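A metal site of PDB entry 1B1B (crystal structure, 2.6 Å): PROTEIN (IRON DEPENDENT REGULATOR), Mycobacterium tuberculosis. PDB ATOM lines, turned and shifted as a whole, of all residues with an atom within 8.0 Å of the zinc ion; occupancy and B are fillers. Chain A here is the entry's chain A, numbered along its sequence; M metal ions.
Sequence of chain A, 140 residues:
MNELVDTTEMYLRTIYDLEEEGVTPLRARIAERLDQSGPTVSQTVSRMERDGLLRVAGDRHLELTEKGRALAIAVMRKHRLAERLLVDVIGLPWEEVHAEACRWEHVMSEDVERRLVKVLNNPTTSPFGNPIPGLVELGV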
ATOM      1  N   ASN A   2     -13.508  -6.929   6.237  1.00  0.00           N
ATOM      2  CA  ASN A   2     -13.491  -8.191   5.506  1.00  0.00           C
ATOM      3  C   ASN A   2     -12.137  -8.474   4.916  1.00  0.00           C
ATOM      4  O   ASN A   2     -12.039  -8.822   3.735  1.00  0.00           O
ATOM      5  CB  ASN A   2     -14.557  -8.183   4.403  1.00  0.00           C
ATOM      6  CG  ASN A   2     -15.921  -7.827   4.930  1.00  0.00           C
ATOM      7  OD1 ASN A   2     -16.517  -6.844   4.493  1.00  0.00           O
ATOM      8  ND2 ASN A   2     -16.370  -8.575   5.921  1.00  0.00           N
ATOM      9  N   GLU A   3     -11.089  -8.280   5.710  1.00  0.00           N
ATOM     10  CA  GLU A   3      -9.728  -8.527   5.263  1.00  0.00           C
ATOM     11  C   GLU A   3      -9.254  -7.459   4.295  1.00  0.00           C
ATOM     12  O   GLU A   3      -8.073  -7.337   4.005  1.00  0.00           O
ATOM     13  CB  GLU A   3      -9.597  -9.934   4.698  1.00  0.00           C
ATOM     14  CG  GLU A   3      -9.726 -11.083   5.737  1.00  0.00           C
ATOM     15  CD  GLU A   3     -10.977 -11.002   6.598  1.00  0.00           C
ATOM     16  OE1 GLU A   3     -12.031 -11.554   6.195  1.00  0.00           O
ATOM     17  OE2 GLU A   3     -10.928 -10.369   7.688  1.00  0.00           O
ATOM     18  N   LEU A   4     -10.213  -6.691   3.778  1.00  0.00           N
ATOM     19  CA  LEU A   4      -9.953  -5.571   2.878  1.00  0.00           C
ATOM     20  C   LEU A   4     -10.348  -4.446   3.836  1.00  0.00           C
ATOM     21  O   LEU A   4     -11.192  -3.598   3.542  1.00  0.00           O
ATOM     22  CB  LEU A   4     -10.896  -5.602   1.684  1.00  0.00           C
ATOM     23  N   VAL A   5      -9.720  -4.471   5.019  1.00  0.00           N
ATOM     24  CA  VAL A   5      -9.992  -3.536   6.093  1.00  0.00           C
ATOM     25  C   VAL A   5      -9.926  -2.045   5.749  1.00  0.00           C
ATOM     26  O   VAL A   5     -10.395  -1.208   6.520  1.00  0.00           O
ATOM     27  CB  VAL A   5      -9.162  -3.895   7.405  1.00  0.00           C
ATOM     28  CG1 VAL A   5      -9.334  -5.368   7.743  1.00  0.00           C
ATOM     29  CG2 VAL A   5      -7.729  -3.632   7.210  1.00  0.00           C
ATOM     30  N   ASP A   6      -9.421  -1.741   4.559  1.00  0.00           N
ATOM     31  CA  ASP A   6      -9.311  -0.363   4.084  1.00  0.00           C
ATOM     32  C   ASP A   6      -9.381  -0.391   2.554  1.00  0.00           C
ATOM     33  O   ASP A   6      -8.383  -0.701   1.880  1.00  0.00           O
ATOM     34  CB  ASP A   6      -7.982   0.273   4.548  1.00  0.00           C
ATOM     35  CG  ASP A   6      -7.975   1.791   4.476  1.00  0.00           C
ATOM     36  OD1 ASP A   6      -8.721   2.405   3.676  1.00  0.00           O
ATOM     37  OD2 ASP A   6      -7.199   2.407   5.246  1.00  0.00           O
ATOM     38  N   THR A   7     -10.555  -0.095   2.012  1.00  0.00           N
ATOM     39  CA  THR A   7     -10.753  -0.102   0.564  1.00  0.00           C
ATOM     40  C   THR A   7      -9.759   0.810  -0.151  1.00  0.00           C
ATOM     41  O   THR A   7      -9.032   0.345  -1.011  1.00  0.00           O
ATOM     42  CB  THR A   7     -12.173   0.312   0.196  1.00  0.00           C
ATOM     43  OG1 THR A   7     -12.360   1.702   0.523  1.00  0.00           O
ATOM     44  CG2 THR A   7     -13.181  -0.534   0.966  1.00  0.00           C
ATOM     45  N   GLU A   9      -6.909   1.853   0.512  1.00  0.00           N
ATOM     46  CA  GLU A   9      -5.571   1.245   0.469  1.00  0.00           C
ATOM     47  C   GLU A   9      -5.561  -0.015  -0.389  1.00  0.00           C
ATOM     48  O   GLU A   9      -4.579  -0.281  -1.091  1.00  0.00           O
ATOM     49  CB  GLU A   9      -5.022   0.981   1.864  1.00  0.00           C
ATOM     50  CG  GLU A   9      -4.837   2.289   2.671  1.00  0.00           C
ATOM     51  CD  GLU A   9      -4.201   2.071   4.050  1.00  0.00           C
ATOM     52  OE1 GLU A   9      -4.601   1.125   4.767  1.00  0.00           O
ATOM     53  OE2 GLU A   9      -3.347   2.876   4.428  1.00  0.00           O
ATOM     54  N   MET A  10      -6.668  -0.767  -0.389  1.00  0.00           N
ATOM     55  CA  MET A  10      -6.722  -1.977  -1.202  1.00  0.00           C
ATOM     56  C   MET A  10      -6.636  -1.652  -2.679  1.00  0.00           C
ATOM     57  O   MET A  10      -5.814  -2.214  -3.388  1.00  0.00           O
ATOM     58  CB  MET A  10      -7.969  -2.785  -0.914  1.00  0.00           C
ATOM     59  CG  MET A  10      -7.855  -3.636   0.342  1.00  0.00           C
ATOM     60  SD  MET A  10      -6.201  -4.458   0.580  1.00  0.00           S
ATOM     61  CE  MET A  10      -5.858  -5.035  -1.142  1.00  0.00           C
ATOM     62  N   ARG A  13      -3.275  -0.558  -3.553  1.00  0.00           N
ATOM     63  CA  ARG A  13      -2.398  -1.712  -3.440  1.00  0.00           C
ATOM     64  C   ARG A  13      -2.518  -2.613  -4.669  1.00  0.00           C
ATOM     65  O   ARG A  13      -1.535  -2.854  -5.373  1.00  0.00           O
ATOM     66  CB  ARG A  13      -2.737  -2.484  -2.160  1.00  0.00           C
ATOM     67  CG  ARG A  13      -1.535  -3.080  -1.454  1.00  0.00           C
ATOM     68  CD  ARG A  13      -1.092  -4.401  -2.083  1.00  0.00           C
ATOM     69  NE  ARG A  13      -1.298  -5.539  -1.196  1.00  0.00           N
ATOM     70  CZ  ARG A  13      -2.046  -6.604  -1.471  1.00  0.00           C
ATOM     71  NH1 ARG A  13      -2.661  -6.721  -2.618  1.00  0.00           N
ATOM     72  NH2 ARG A  13      -2.157  -7.584  -0.574  1.00  0.00           N
ATOM     73  N   THR A  14      -3.744  -3.068  -4.936  1.00  0.00           N
ATOM     74  CA  THR A  14      -4.012  -3.934  -6.078  1.00  0.00           C
ATOM     75  C   THR A  14      -3.391  -3.437  -7.391  1.00  0.00           C
ATOM     76  O   THR A  14      -3.029  -4.240  -8.236  1.00  0.00           O
ATOM     77  CB  THR A  14      -5.522  -4.121  -6.254  1.00  0.00           C
ATOM     78  OG1 THR A  14      -6.040  -4.910  -5.136  1.00  0.00           O
ATOM     79  CG2 THR A  14      -5.844  -4.803  -7.573  1.00  0.00           C
ATOM     80  N   LEU A  34     -10.892  -7.778  -5.953  1.00  0.00           N
ATOM     81  CA  LEU A  34     -11.412  -7.337  -4.662  1.00  0.00           C
ATOM     82  C   LEU A  34     -12.863  -7.718  -4.416  1.00  0.00           C
ATOM     83  O   LEU A  34     -13.410  -7.430  -3.363  1.00  0.00           O
ATOM     84  CB  LEU A  34     -11.247  -5.824  -4.545  1.00  0.00           C
ATOM     85  CG  LEU A  34      -9.863  -5.235  -4.819  1.00  0.00           C
ATOM     86  CD1 LEU A  34      -9.914  -3.730  -4.758  1.00  0.00           C
ATOM     87  CD2 LEU A  34      -8.851  -5.761  -3.814  1.00  0.00           C
ATOM     88  N   VAL A  75       1.869   0.757   2.248  1.00  0.00           N
ATOM     89  CA  VAL A  75       0.989  -0.353   2.615  1.00  0.00           C
ATOM     90  C   VAL A  75       1.659  -1.677   2.181  1.00  0.00           C
ATOM     91  O   VAL A  75       1.509  -2.706   2.849  1.00  0.00           O
ATOM     92  CB  VAL A  75      -0.396  -0.189   1.944  1.00  0.00           C
ATOM     93  CG1 VAL A  75      -1.285  -1.397   2.216  1.00  0.00           C
ATOM     94  CG2 VAL A  75      -1.044   1.103   2.403  1.00  0.00           C
ATOM     95  N   HIS A  79       2.747  -4.456   4.615  1.00  0.00           N
ATOM     96  CA  HIS A  79       2.310  -5.780   4.220  1.00  0.00           C
ATOM     97  C   HIS A  79       3.473  -6.757   4.327  1.00  0.00           C
ATOM     98  O   HIS A  79       3.441  -7.728   5.090  1.00  0.00           O
ATOM     99  CB  HIS A  79       1.836  -5.702   2.767  1.00  0.00           C
ATOM    100  CG  HIS A  79       1.351  -6.992   2.209  1.00  0.00           C
ATOM    101  ND1 HIS A  79       0.027  -7.203   1.948  1.00  0.00           N
ATOM    102  CD2 HIS A  79       2.033  -8.146   2.011  1.00  0.00           C
ATOM    103  CE1 HIS A  79      -0.069  -8.470   1.592  1.00  0.00           C
ATOM    104  NE2 HIS A  79       1.106  -9.103   1.602  1.00  0.00           N
ATOM    105  N   HIS A  98       0.179 -14.700   4.068  1.00  0.00           N
ATOM    106  CA  HIS A  98      -0.384 -13.694   3.155  1.00  0.00           C
ATOM    107  C   HIS A  98      -1.712 -13.066   3.557  1.00  0.00           C
ATOM    108  O   HIS A  98      -1.823 -11.839   3.555  1.00  0.00           O
ATOM    109  CB  HIS A  98      -0.543 -14.275   1.752  1.00  0.00           C
ATOM    110  CG  HIS A  98      -1.152 -13.293   0.778  1.00  0.00           C
ATOM    111  ND1 HIS A  98      -0.432 -12.199   0.322  1.00  0.00           N
ATOM    112  CD2 HIS A  98      -2.367 -13.272   0.221  1.00  0.00           C
ATOM    113  CE1 HIS A  98      -1.235 -11.586  -0.512  1.00  0.00           C
ATOM    114  NE2 HIS A  98      -2.416 -12.181  -0.614  1.00  0.00           N
ATOM    115  N   ALA A  99      -2.716 -13.919   3.773  1.00  0.00           N
ATOM    116  CA  ALA A  99      -4.038 -13.445   4.153  1.00  0.00           C
ATOM    117  C   ALA A  99      -3.994 -12.698   5.482  1.00  0.00           C
ATOM    118  O   ALA A  99      -4.797 -11.817   5.719  1.00  0.00           O
ATOM    119  CB  ALA A  99      -5.007 -14.583   4.234  1.00  0.00           C
ATOM    120  N   GLU A 100      -3.024 -13.066   6.307  1.00  0.00           N
ATOM    121  CA  GLU A 100      -2.814 -12.431   7.614  1.00  0.00           C
ATOM    122  C   GLU A 100      -2.252 -11.025   7.428  1.00  0.00           C
ATOM    123  O   GLU A 100      -2.822 -10.040   7.918  1.00  0.00           O
ATOM    124  CB  GLU A 100      -1.875 -13.274   8.483  1.00  0.00           C
ATOM    125  CG  GLU A 100      -1.713 -12.775   9.928  1.00  0.00           C
ATOM    126  CD  GLU A 100      -2.853 -13.194  10.834  1.00  0.00           C
ATOM    127  OE1 GLU A 100      -3.356 -14.308  10.682  1.00  0.00           O
ATOM    128  OE2 GLU A 100      -3.266 -12.403  11.705  1.00  0.00           O
ATOM    129  N   ALA A 101      -1.124 -10.928   6.703  1.00  0.00           N
ATOM    130  CA  ALA A 101      -0.448  -9.668   6.413  1.00  0.00           C
ATOM    131  C   ALA A 101      -1.339  -8.742   5.582  1.00  0.00           C
ATOM    132  O   ALA A 101      -1.221  -7.521   5.675  1.00  0.00           O
ATOM    133  CB  ALA A 101       0.826  -9.935   5.685  1.00  0.00           C
ATOM    134  N   CYS A 102      -2.246  -9.343   4.802  1.00  0.00           N
ATOM    135  CA  CYS A 102      -3.210  -8.642   3.947  1.00  0.00           C
ATOM    136  C   CYS A 102      -4.097  -7.710   4.820  1.00  0.00           C
ATOM    137  O   CYS A 102      -4.631  -6.707   4.341  1.00  0.00           O
ATOM    138  CB  CYS A 102      -4.054  -9.685   3.194  1.00  0.00           C
ATOM    139  SG  CYS A 102      -5.075  -9.117   1.783  1.00  0.00           S
ATOM    140  N   ARG A 103      -4.241  -8.048   6.096  1.00  0.00           N
ATOM    141  CA  ARG A 103      -5.033  -7.265   7.025  1.00  0.00           C
ATOM    142  C   ARG A 103      -4.162  -6.338   7.869  1.00  0.00           C
ATOM    143  O   ARG A 103      -4.362  -5.127   7.894  1.00  0.00           O
ATOM    144  CB  ARG A 103      -5.822  -8.197   7.913  1.00  0.00           C
ATOM    145  CG  ARG A 103      -6.977  -8.804   7.194  1.00  0.00           C
ATOM    146  CD  ARG A 103      -8.029  -9.333   8.131  1.00  0.00           C
ATOM    147  NE  ARG A 103      -7.905 -10.765   8.241  1.00  0.00           N
ATOM    148  CZ  ARG A 103      -7.173 -11.352   9.167  1.00  0.00           C
ATOM    149  NH1 ARG A 103      -6.525 -10.598  10.043  1.00  0.00           N
ATOM    150  NH2 ARG A 103      -7.060 -12.673   9.231  1.00  0.00           N
ATOM    151  N   TRP A 104      -3.200  -6.933   8.558  1.00  0.00           N
ATOM    152  CA  TRP A 104      -2.290  -6.198   9.432  1.00  0.00           C
ATOM    153  C   TRP A 104      -1.671  -5.006   8.723  1.00  0.00           C
ATOM    154  O   TRP A 104      -1.388  -3.993   9.343  1.00  0.00           O
ATOM    155  CB  TRP A 104      -1.191  -7.114   9.983  1.00  0.00           C
ATOM    156  CG  TRP A 104      -1.706  -8.164  10.958  1.00  0.00           C
ATOM    157  CD1 TRP A 104      -2.991  -8.580  11.128  1.00  0.00           C
ATOM    158  CD2 TRP A 104      -0.912  -8.926  11.873  1.00  0.00           C
ATOM    159  NE1 TRP A 104      -3.041  -9.552  12.088  1.00  0.00           N
ATOM    160  CE2 TRP A 104      -1.781  -9.789  12.570  1.00  0.00           C
ATOM    161  CE3 TRP A 104       0.460  -8.975  12.178  1.00  0.00           C
ATOM    162  CZ2 TRP A 104      -1.345 -10.699  13.534  1.00  0.00           C
ATOM    163  CZ3 TRP A 104       0.907  -9.869  13.131  1.00  0.00           C
ATOM    164  CH2 TRP A 104      -0.005 -10.712  13.811  1.00  0.00           C
ATOM    165  N   GLU A 105      -1.514  -5.126   7.400  1.00  0.00           N
ATOM    166  CA  GLU A 105      -0.936  -4.047   6.597  1.00  0.00           C
ATOM    167  C   GLU A 105      -1.665  -2.723   6.763  1.00  0.00           C
ATOM    168  O   GLU A 105      -1.050  -1.651   6.668  1.00  0.00           O
ATOM    169  CB  GLU A 105      -0.908  -4.436   5.099  1.00  0.00           C
ATOM    170  CG  GLU A 105      -2.238  -4.889   4.562  1.00  0.00           C
ATOM    171  CD  GLU A 105      -2.254  -5.039   3.014  1.00  0.00           C
ATOM    172  OE1 GLU A 105      -1.204  -5.056   2.381  1.00  0.00           O
ATOM    173  OE2 GLU A 105      -3.461  -5.162   2.501  1.00  0.00           O
ATOM    174  N   HIS A 106      -2.985  -2.775   7.013  1.00  0.00           N
ATOM    175  CA  HIS A 106      -3.771  -1.557   7.164  1.00  0.00           C
ATOM    176  C   HIS A 106      -3.726  -1.018   8.569  1.00  0.00           C
ATOM    177  O   HIS A 106      -4.221   0.088   8.832  1.00  0.00           O
ATOM    178  CB  HIS A 106      -5.238  -1.778   6.778  1.00  0.00           C
ATOM    179  CG  HIS A 106      -5.433  -2.341   5.398  1.00  0.00           C
ATOM    180  ND1 HIS A 106      -5.443  -1.518   4.291  1.00  0.00           N
ATOM    181  CD2 HIS A 106      -5.610  -3.613   5.003  1.00  0.00           C
ATOM    182  CE1 HIS A 106      -5.627  -2.331   3.270  1.00  0.00           C
ATOM    183  NE2 HIS A 106      -5.732  -3.604   3.619  1.00  0.00           N
HETATM  184 ZN    ZN M   1      -5.184  -5.746   2.689  1.00  0.00          ZN
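The zinc ion is bound by OE2 of Glu 105, O of Cys 102, NE2 of His 106 and SD of Met 10.
The zinc ion has four donor atoms within binding distance.
Residues that only touch the zinc ion: Glu 3 (3.6 Å).
Of the 22 residues printed, 5 come within 4 Å of the zinc ion.
The nearest printed residue that does not touch the zinc ion is Arg 103 (4.2 Å).
The guanidinium group (NE) of Arg 13 lies within salt-bridge range of the side-chain carboxylate (OE1) of Glu 105 (3.6 Å).
A ring nitrogen (ND1) of His 79 sits at hydrogen-bond distance from the side-chain carboxylate of Glu 105, at 2.5 Å.
A ring nitrogen (ND1) of His 106 is in hydrogen-bond range of the side-chain carboxylate of Glu 9 (2.8 Å).
The backbone carbonyl oxygen (O) of Met 10 sits at hydrogen-bond distance from the side-chain hydroxyl (OG1) of Thr 14, 3.2 Å away.
The side-chain carboxylate (OE2) of Glu 3 is in salt-bridge range of the guanidinium group (NE) of Arg 103 (3.1 Å).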
